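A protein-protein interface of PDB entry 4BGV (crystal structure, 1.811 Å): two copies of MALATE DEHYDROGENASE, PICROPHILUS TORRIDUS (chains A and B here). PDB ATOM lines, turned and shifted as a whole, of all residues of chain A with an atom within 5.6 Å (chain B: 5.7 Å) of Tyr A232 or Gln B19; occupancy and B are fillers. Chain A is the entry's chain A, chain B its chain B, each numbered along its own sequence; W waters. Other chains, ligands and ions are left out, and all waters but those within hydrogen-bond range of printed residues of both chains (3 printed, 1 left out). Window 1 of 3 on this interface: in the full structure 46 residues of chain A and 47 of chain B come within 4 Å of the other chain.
The backbone NH of Tyr A232 is in hydrogen-bond range of the side-chain carboxylate of Asp B45.
The side-chain hydroxyl of Tyr A225 is in hydrogen-bond range of the side-chain carboxylate of Asp B45 (2.8 Å).
N of Phe A231 sits at hydrogen-bond distance from OD2 of Asp B45 (2.9 Å).
N of Ala A233 is in hydrogen-bond range of OD1 of Asp B45 (2.9 Å).
Hydrophobic or aromatic side chains of chain A that line the printed part of chain B: Tyr A225, Ala A230, Phe A231, Tyr A232, Ala A233, Pro A234 and Ile A236.
Hydrophobic or aromatic side chains of chain B that line the printed part of chain A: Ala B15, Ile B46 and Trp B53.
Along chain B the printed residues that touch a printed residue of chain A span positions 15 to 53.
Position printed for both chains: 16.
Of the 14 pairs that touch across the chains among the printed residues, none has its exchanged pair printed and touching as well.
Among the printed residues, merely in contact across the chains: Tyr A232 with Gln B19 (3.4 Å), Ile A236 with Trp B53 (3.4 Å), Tyr A225 with Lys B42 (3.5 Å), Tyr A232 with Ala B15 (3.5 Å), Ala A230 with Asp B45 (3.6 Å), Tyr A232 with Thr B16 (3.6 Å), Tyr A232 with Ile B46 (3.6 Å), Pro A234 with Asp B45 (3.7 Å), Ile A236 with Gly B49 (3.7 Å) and Ala A233 with Gly B49 (3.9 Å).
Water W1 lies within hydrogen-bond range of the side-chain hydroxyl of Thr B16 (2.6 Å) and the side-chain hydroxyl of Tyr A232 (2.7 Å).
Water W2 lies within hydrogen-bond range of the side-chain amide oxygen of Gln B19 (2.8 Å), the backbone carbonyl oxygen of Tyr A232 (2.8 Å) and the indole nitrogen of Trp B53 (3.0 Å).
Water W3 bridges the side-chain amino group (NZ) of Lys B42 and the side-chain hydroxyl (OH) of Tyr A232.
O of Ala B12 lies within hydrogen-bond range of OG1 of Thr B16 (2.6 Å).
NE2 of Gln B19 is in hydrogen-bond range of OH of Tyr B55 (3.0 Å).
The side-chain hydroxyl of Ser A237 lies within hydrogen-bond range of the backbone carbonyl oxygen of Ala A233 (2.8 Å).
The side-chain hydroxyl of Tyr B55 lies within hydrogen-bond range of the backbone carbonyl oxygen of Ile B46 (2.6 Å).
The side-chain hydroxyl of Thr B20 is in hydrogen-bond range of the backbone carbonyl oxygen of Thr B16 (2.7 Å).
Of the printed residues of chain B, Ala A230 touches Asp B45 (3.6 Å).
Printed residues of chain B within 4 Å of Tyr A232: Ala B15, Thr B16, Gln B19, Asp B45 and Ile B46.
Printed residues of chain B within 4 Å of Ile A236: Gly B49 and Trp B53.
Printed residues of chain A within 4 Å of Ala B15: Tyr A232.
Of chain A, only Tyr A232 comes within 4 Å of Gln B19.
Of the printed residues of chain A, Lys B42 touches Tyr A225 (3.5 Å).
Of the printed residues of chain A, Asp B45 touches Tyr A225, Ala A230, Phe A231, Tyr A232, Ala A233 and Pro A234.
The nearest printed residue of chain B that does not touch Phe A231 is Lys B42 (4.1 Å).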
ATOM      1  N   THR A  16       0.442  -7.648  14.266  1.00  0.00           N
ATOM      2  CA  THR A  16       1.146  -8.616  13.424  1.00  0.00           C
ATOM      3  C   THR A  16       1.819  -9.654  14.312  1.00  0.00           C
ATOM      4  O   THR A  16       1.790 -10.846  14.019  1.00  0.00           O
ATOM      5  CB  THR A  16       2.190  -7.917  12.532  1.00  0.00           C
ATOM      6  OG1 THR A  16       1.504  -6.996  11.681  1.00  0.00           O
ATOM      7  CG2 THR A  16       2.947  -8.918  11.639  1.00  0.00           C
ATOM      8  N   TYR A 225       5.791   3.013   2.248  1.00  0.00           N
ATOM      9  CA  TYR A 225       4.493   3.078   2.935  1.00  0.00           C
ATOM     10  C   TYR A 225       3.955   4.506   3.075  1.00  0.00           C
ATOM     11  O   TYR A 225       2.737   4.713   3.153  1.00  0.00           O
ATOM     12  CB  TYR A 225       4.600   2.476   4.340  1.00  0.00           C
ATOM     13  CG  TYR A 225       4.593   0.962   4.402  1.00  0.00           C
ATOM     14  CD1 TYR A 225       4.275   0.192   3.282  1.00  0.00           C
ATOM     15  CD2 TYR A 225       4.867   0.302   5.600  1.00  0.00           C
ATOM     16  CE1 TYR A 225       4.255  -1.197   3.358  1.00  0.00           C
ATOM     17  CE2 TYR A 225       4.851  -1.083   5.681  1.00  0.00           C
ATOM     18  CZ  TYR A 225       4.539  -1.822   4.552  1.00  0.00           C
ATOM     19  OH  TYR A 225       4.505  -3.199   4.615  1.00  0.00           O
ATOM     20  N   ALA A 230       7.602  -0.384   8.786  1.00  0.00           N
ATOM     21  CA  ALA A 230       7.544  -1.834   8.551  1.00  0.00           C
ATOM     22  C   ALA A 230       6.816  -2.559   9.681  1.00  0.00           C
ATOM     23  O   ALA A 230       6.899  -2.147  10.846  1.00  0.00           O
ATOM     24  CB  ALA A 230       8.959  -2.396   8.398  1.00  0.00           C
ATOM     25  N   PHE A 231       6.120  -3.644   9.343  1.00  0.00           N
ATOM     26  CA  PHE A 231       5.473  -4.461  10.359  1.00  0.00           C
ATOM     27  C   PHE A 231       5.504  -5.973  10.101  1.00  0.00           C
ATOM     28  O   PHE A 231       5.551  -6.746  11.046  1.00  0.00           O
ATOM     29  CB  PHE A 231       4.042  -3.982  10.678  1.00  0.00           C
ATOM     30  CG  PHE A 231       3.135  -3.911   9.490  1.00  0.00           C
ATOM     31  CD1 PHE A 231       3.176  -2.809   8.632  1.00  0.00           C
ATOM     32  CD2 PHE A 231       2.209  -4.926   9.245  1.00  0.00           C
ATOM     33  CE1 PHE A 231       2.309  -2.729   7.539  1.00  0.00           C
ATOM     34  CE2 PHE A 231       1.342  -4.852   8.154  1.00  0.00           C
ATOM     35  CZ  PHE A 231       1.392  -3.758   7.296  1.00  0.00           C
ATOM     36  N   TYR A 232       5.485  -6.394   8.842  1.00  0.00           N
ATOM     37  CA  TYR A 232       5.524  -7.831   8.562  1.00  0.00           C
ATOM     38  C   TYR A 232       6.841  -8.483   8.966  1.00  0.00           C
ATOM     39  O   TYR A 232       6.849  -9.473   9.711  1.00  0.00           O
ATOM     40  CB  TYR A 232       5.227  -8.130   7.087  1.00  0.00           C
ATOM     41  CG  TYR A 232       3.776  -7.920   6.721  1.00  0.00           C
ATOM     42  CD1 TYR A 232       2.773  -8.706   7.312  1.00  0.00           C
ATOM     43  CD2 TYR A 232       3.400  -6.942   5.800  1.00  0.00           C
ATOM     44  CE1 TYR A 232       1.439  -8.530   6.985  1.00  0.00           C
ATOM     45  CE2 TYR A 232       2.050  -6.758   5.457  1.00  0.00           C
ATOM     46  CZ  TYR A 232       1.085  -7.551   6.057  1.00  0.00           C
ATOM     47  OH  TYR A 232      -0.247  -7.372   5.755  1.00  0.00           O
ATOM     48  N   ALA A 233       7.951  -7.964   8.455  1.00  0.00           N
ATOM     49  CA  ALA A 233       9.253  -8.527   8.821  1.00  0.00           C
ATOM     50  C   ALA A 233       9.576  -8.333  10.318  1.00  0.00           C
ATOM     51  O   ALA A 233      10.019  -9.279  10.978  1.00  0.00           O
ATOM     52  CB  ALA A 233      10.374  -7.994   7.919  1.00  0.00           C
ATOM     53  N   PRO A 234       9.323  -7.121  10.868  1.00  0.00           N
ATOM     54  CA  PRO A 234       9.446  -6.997  12.325  1.00  0.00           C
ATOM     55  C   PRO A 234       8.573  -8.013  13.070  1.00  0.00           C
ATOM     56  O   PRO A 234       9.053  -8.619  14.017  1.00  0.00           O
ATOM     57  CB  PRO A 234       8.938  -5.578  12.589  1.00  0.00           C
ATOM     58  CG  PRO A 234       9.314  -4.822  11.331  1.00  0.00           C
ATOM     59  CD  PRO A 234       9.044  -5.813  10.233  1.00  0.00           C
ATOM     60  N   GLY A 235       7.341  -8.233  12.629  1.00  0.00           N
ATOM     61  CA  GLY A 235       6.460  -9.162  13.327  1.00  0.00           C
ATOM     62  C   GLY A 235       7.034 -10.566  13.511  1.00  0.00           C
ATOM     63  O   GLY A 235       7.011 -11.124  14.611  1.00  0.00           O
ATOM     64  N   ILE A 236       7.557 -11.148  12.437  1.00  0.00           N
ATOM     65  CA  ILE A 236       8.153 -12.479  12.551  1.00  0.00           C
ATOM     66  C   ILE A 236       9.507 -12.423  13.278  1.00  0.00           C
ATOM     67  O   ILE A 236       9.846 -13.337  14.016  1.00  0.00           O
ATOM     68  CB  ILE A 236       8.220 -13.234  11.178  1.00  0.00           C
ATOM     69  CG1 ILE A 236       8.783 -14.655  11.352  1.00  0.00           C
ATOM     70  CG2 ILE A 236       9.016 -12.438  10.108  1.00  0.00           C
ATOM     71  CD1 ILE A 236       7.913 -15.562  12.198  1.00  0.00           C
ATOM     72  N   SER A 237      10.257 -11.336  13.110  1.00  0.00           N
ATOM     73  CA  SER A 237      11.544 -11.190  13.813  1.00  0.00           C
ATOM     74  C   SER A 237      11.349 -11.182  15.334  1.00  0.00           C
ATOM     75  O   SER A 237      12.153 -11.731  16.086  1.00  0.00           O
ATOM     76  CB  SER A 237      12.264  -9.906  13.370  1.00  0.00           C
ATOM     77  OG  SER A 237      12.547  -9.952  11.982  1.00  0.00           O
ATOM     78  N   ALA B  12      -4.971  -3.312   3.587  1.00  0.00           N
ATOM     79  CA  ALA B  12      -4.978  -4.328   4.654  1.00  0.00           C
ATOM     80  C   ALA B  12      -5.398  -5.705   4.143  1.00  0.00           C
ATOM     81  O   ALA B  12      -4.722  -6.715   4.412  1.00  0.00           O
ATOM     82  CB  ALA B  12      -5.882  -3.887   5.805  1.00  0.00           C
ATOM     83  N   GLY B  14      -5.635  -7.040   0.865  1.00  0.00           N
ATOM     84  CA  GLY B  14      -4.757  -7.605  -0.156  1.00  0.00           C
ATOM     85  C   GLY B  14      -3.383  -8.007   0.358  1.00  0.00           C
ATOM     86  O   GLY B  14      -2.845  -9.057  -0.006  1.00  0.00           O
ATOM     87  N   ALA B  15      -2.789  -7.157   1.185  1.00  0.00           N
ATOM     88  CA  ALA B  15      -1.480  -7.472   1.755  1.00  0.00           C
ATOM     89  C   ALA B  15      -1.582  -8.648   2.728  1.00  0.00           C
ATOM     90  O   ALA B  15      -0.665  -9.473   2.802  1.00  0.00           O
ATOM     91  CB  ALA B  15      -0.862  -6.241   2.438  1.00  0.00           C
ATOM     92  N   THR B  16      -2.694  -8.746   3.460  1.00  0.00           N
ATOM     93  CA  THR B  16      -2.894  -9.893   4.363  1.00  0.00           C
ATOM     94  C   THR B  16      -2.997 -11.168   3.541  1.00  0.00           C
ATOM     95  O   THR B  16      -2.437 -12.199   3.914  1.00  0.00           O
ATOM     96  CB  THR B  16      -4.153  -9.753   5.260  1.00  0.00           C
ATOM     97  OG1 THR B  16      -4.010  -8.609   6.107  1.00  0.00           O
ATOM     98  CG2 THR B  16      -4.355 -11.009   6.153  1.00  0.00           C
ATOM     99  N   VAL B  17      -3.700 -11.097   2.411  1.00  0.00           N
ATOM    100  CA  VAL B  17      -3.764 -12.258   1.519  1.00  0.00           C
ATOM    101  C   VAL B  17      -2.339 -12.642   1.092  1.00  0.00           C
ATOM    102  O   VAL B  17      -1.961 -13.817   1.126  1.00  0.00           O
ATOM    103  CB  VAL B  17      -4.669 -11.994   0.300  1.00  0.00           C
ATOM    104  CG1 VAL B  17      -4.539 -13.108  -0.743  1.00  0.00           C
ATOM    105  CG2 VAL B  17      -6.129 -11.834   0.749  1.00  0.00           C
ATOM    106  N   ALA B  18      -1.538 -11.655   0.720  1.00  0.00           N
ATOM    107  CA  ALA B  18      -0.195 -11.941   0.216  1.00  0.00           C
ATOM    108  C   ALA B  18       0.658 -12.561   1.305  1.00  0.00           C
ATOM    109  O   ALA B  18       1.382 -13.527   1.057  1.00  0.00           O
ATOM    110  CB  ALA B  18       0.470 -10.663  -0.347  1.00  0.00           C
ATOM    111  N   GLN B  19       0.584 -12.015   2.520  1.00  0.00           N
ATOM    112  CA  GLN B  19       1.399 -12.562   3.604  1.00  0.00           C
ATOM    113  C   GLN B  19       0.945 -13.979   3.930  1.00  0.00           C
ATOM    114  O   GLN B  19       1.761 -14.857   4.201  1.00  0.00           O
ATOM    115  CB  GLN B  19       1.373 -11.651   4.850  1.00  0.00           C
ATOM    116  CG  GLN B  19       2.119 -12.236   6.081  1.00  0.00           C
ATOM    117  CD  GLN B  19       3.626 -12.357   5.857  1.00  0.00           C
ATOM    118  OE1 GLN B  19       4.397 -11.454   6.219  1.00  0.00           O
ATOM    119  NE2 GLN B  19       4.054 -13.475   5.255  1.00  0.00           N
ATOM    120  N   THR B  20      -0.363 -14.200   3.885  1.00  0.00           N
ATOM    121  CA  THR B  20      -0.932 -15.516   4.177  1.00  0.00           C
ATOM    122  C   THR B  20      -0.495 -16.539   3.118  1.00  0.00           C
ATOM    123  O   THR B  20      -0.057 -17.643   3.457  1.00  0.00           O
ATOM    124  CB  THR B  20      -2.475 -15.443   4.250  1.00  0.00           C
ATOM    125  OG1 THR B  20      -2.866 -14.530   5.287  1.00  0.00           O
ATOM    126  CG2 THR B  20      -3.076 -16.828   4.555  1.00  0.00           C
ATOM    127  N   LEU B  21      -0.608 -16.181   1.837  1.00  0.00           N
ATOM    128  CA  LEU B  21      -0.143 -17.076   0.756  1.00  0.00           C
ATOM    129  C   LEU B  21       1.347 -17.422   0.863  1.00  0.00           C
ATOM    130  O   LEU B  21       1.748 -18.552   0.567  1.00  0.00           O
ATOM    131  CB  LEU B  21      -0.411 -16.469  -0.630  1.00  0.00           C
ATOM    132  CG  LEU B  21      -1.888 -16.302  -1.028  1.00  0.00           C
ATOM    133  CD1 LEU B  21      -1.992 -15.501  -2.333  1.00  0.00           C
ATOM    134  CD2 LEU B  21      -2.590 -17.648  -1.172  1.00  0.00           C
ATOM    135  N   ALA B  22       2.159 -16.452   1.288  1.00  0.00           N
ATOM    136  CA  ALA B  22       3.589 -16.701   1.481  1.00  0.00           C
ATOM    137  C   ALA B  22       3.830 -17.699   2.611  1.00  0.00           C
ATOM    138  O   ALA B  22       4.581 -18.650   2.442  1.00  0.00           O
ATOM    139  CB  ALA B  22       4.339 -15.398   1.754  1.00  0.00           C
ATOM    140  N   ILE B  23       3.194 -17.477   3.761  1.00  0.00           N
ATOM    141  CA  ILE B  23       3.313 -18.409   4.892  1.00  0.00           C
ATOM    142  C   ILE B  23       2.920 -19.832   4.505  1.00  0.00           C
ATOM    143  O   ILE B  23       3.585 -20.813   4.871  1.00  0.00           O
ATOM    144  CB  ILE B  23       2.471 -17.924   6.077  1.00  0.00           C
ATOM    145  CG1 ILE B  23       3.115 -16.666   6.667  1.00  0.00           C
ATOM    146  CG2 ILE B  23       2.336 -19.027   7.146  1.00  0.00           C
ATOM    147  CD1 ILE B  23       2.151 -15.845   7.512  1.00  0.00           C
ATOM    148  N   ARG B  24       1.835 -19.938   3.748  1.00  0.00           N
ATOM    149  CA  ARG B  24       1.323 -21.233   3.328  1.00  0.00           C
ATOM    150  C   ARG B  24       2.041 -21.736   2.071  1.00  0.00           C
ATOM    151  O   ARG B  24       1.723 -22.815   1.556  1.00  0.00           O
ATOM    152  CB  ARG B  24      -0.195 -21.146   3.155  1.00  0.00           C
ATOM    153  CG  ARG B  24      -0.890 -20.827   4.483  1.00  0.00           C
ATOM    154  CD  ARG B  24      -2.392 -20.628   4.321  1.00  0.00           C
ATOM    155  NE  ARG B  24      -3.133 -21.875   4.083  1.00  0.00           N
ATOM    156  CZ  ARG B  24      -3.596 -22.676   5.041  1.00  0.00           C
ATOM    157  NH1 ARG B  24      -3.349 -22.414   6.322  1.00  0.00           N
ATOM    158  NH2 ARG B  24      -4.295 -23.761   4.717  1.00  0.00           N
ATOM    159  N   LYS B  42       4.587  -3.314   0.643  1.00  0.00           N
ATOM    160  CA  LYS B  42       3.992  -4.509   1.246  1.00  0.00           C
ATOM    161  C   LYS B  42       4.737  -5.767   0.783  1.00  0.00           C
ATOM    162  O   LYS B  42       5.040  -6.653   1.585  1.00  0.00           O
ATOM    163  CB  LYS B  42       2.503  -4.621   0.908  1.00  0.00           C
ATOM    164  CG  LYS B  42       1.624  -3.489   1.467  1.00  0.00           C
ATOM    165  CD  LYS B  42       1.464  -3.548   2.990  1.00  0.00           C
ATOM    166  CE  LYS B  42       0.558  -2.419   3.503  1.00  0.00           C
ATOM    167  NZ  LYS B  42      -0.921  -2.671   3.317  1.00  0.00           N
ATOM    168  N   ASP B  45       8.203  -5.891   2.589  1.00  0.00           N
ATOM    169  CA  ASP B  45       8.062  -6.134   4.019  1.00  0.00           C
ATOM    170  C   ASP B  45       7.770  -7.622   4.212  1.00  0.00           C
ATOM    171  O   ASP B  45       8.366  -8.292   5.052  1.00  0.00           O
ATOM    172  CB  ASP B  45       6.925  -5.253   4.572  1.00  0.00           C
ATOM    173  CG  ASP B  45       6.957  -5.086   6.092  1.00  0.00           C
ATOM    174  OD1 ASP B  45       7.914  -5.543   6.772  1.00  0.00           O
ATOM    175  OD2 ASP B  45       6.001  -4.452   6.607  1.00  0.00           O
ATOM    176  N   ILE B  46       6.876  -8.150   3.389  1.00  0.00           N
ATOM    177  CA  ILE B  46       6.548  -9.565   3.443  1.00  0.00           C
ATOM    178  C   ILE B  46       7.761 -10.426   3.072  1.00  0.00           C
ATOM    179  O   ILE B  46       8.072 -11.423   3.737  1.00  0.00           O
ATOM    180  CB  ILE B  46       5.352  -9.863   2.511  1.00  0.00           C
ATOM    181  CG1 ILE B  46       4.064  -9.292   3.118  1.00  0.00           C
ATOM    182  CG2 ILE B  46       5.177 -11.367   2.311  1.00  0.00           C
ATOM    183  CD1 ILE B  46       2.852  -9.223   2.130  1.00  0.00           C
ATOM    184  N   GLY B  49      10.652 -11.119   5.607  1.00  0.00           N
ATOM    185  CA  GLY B  49      10.438 -12.099   6.661  1.00  0.00           C
ATOM    186  C   GLY B  49      10.704 -13.535   6.224  1.00  0.00           C
ATOM    187  O   GLY B  49      10.685 -14.448   7.053  1.00  0.00           O
ATOM    188  N   TRP B  53      10.561 -17.096   8.284  1.00  0.00           N
ATOM    189  CA  TRP B  53       9.410 -17.969   8.023  1.00  0.00           C
ATOM    190  C   TRP B  53       9.794 -19.238   7.267  1.00  0.00           C
ATOM    191  O   TRP B  53       9.274 -20.323   7.543  1.00  0.00           O
ATOM    192  CB  TRP B  53       8.366 -17.242   7.176  1.00  0.00           C
ATOM    193  CG  TRP B  53       7.412 -16.342   7.929  1.00  0.00           C
ATOM    194  CD1 TRP B  53       7.355 -14.974   7.881  1.00  0.00           C
ATOM    195  CD2 TRP B  53       6.361 -16.753   8.824  1.00  0.00           C
ATOM    196  NE1 TRP B  53       6.333 -14.514   8.674  1.00  0.00           N
ATOM    197  CE2 TRP B  53       5.711 -15.582   9.269  1.00  0.00           C
ATOM    198  CE3 TRP B  53       5.903 -17.995   9.275  1.00  0.00           C
ATOM    199  CZ2 TRP B  53       4.625 -15.617  10.146  1.00  0.00           C
ATOM    200  CZ3 TRP B  53       4.819 -18.026  10.164  1.00  0.00           C
ATOM    201  CH2 TRP B  53       4.204 -16.848  10.582  1.00  0.00           C
ATOM    202  N   TYR B  55       9.846 -19.303   3.598  1.00  0.00           N
ATOM    203  CA  TYR B  55       9.328 -19.368   2.234  1.00  0.00           C
ATOM    204  C   TYR B  55      10.299 -18.888   1.165  1.00  0.00           C
ATOM    205  O   TYR B  55      10.697 -17.729   1.163  1.00  0.00           O
ATOM    206  CB  TYR B  55       7.963 -18.662   2.071  1.00  0.00           C
ATOM    207  CG  TYR B  55       7.759 -17.318   2.769  1.00  0.00           C
ATOM    208  CD1 TYR B  55       8.182 -16.115   2.180  1.00  0.00           C
ATOM    209  CD2 TYR B  55       7.057 -17.243   3.965  1.00  0.00           C
ATOM    210  CE1 TYR B  55       7.959 -14.887   2.815  1.00  0.00           C
ATOM    211  CE2 TYR B  55       6.818 -16.026   4.593  1.00  0.00           C
ATOM    212  CZ  TYR B  55       7.273 -14.854   4.021  1.00  0.00           C
ATOM    213  OH  TYR B  55       7.034 -13.655   4.677  1.00  0.00           O
HETATM  214  O   HOH W   1      -1.793  -8.669   7.539  1.00  0.00           O
HETATM  215  O   HOH W   2       5.385 -11.712   8.820  1.00  0.00           O
HETATM  216  O   HOH W   3      -1.323  -4.734   5.284  1.00  0.00           O
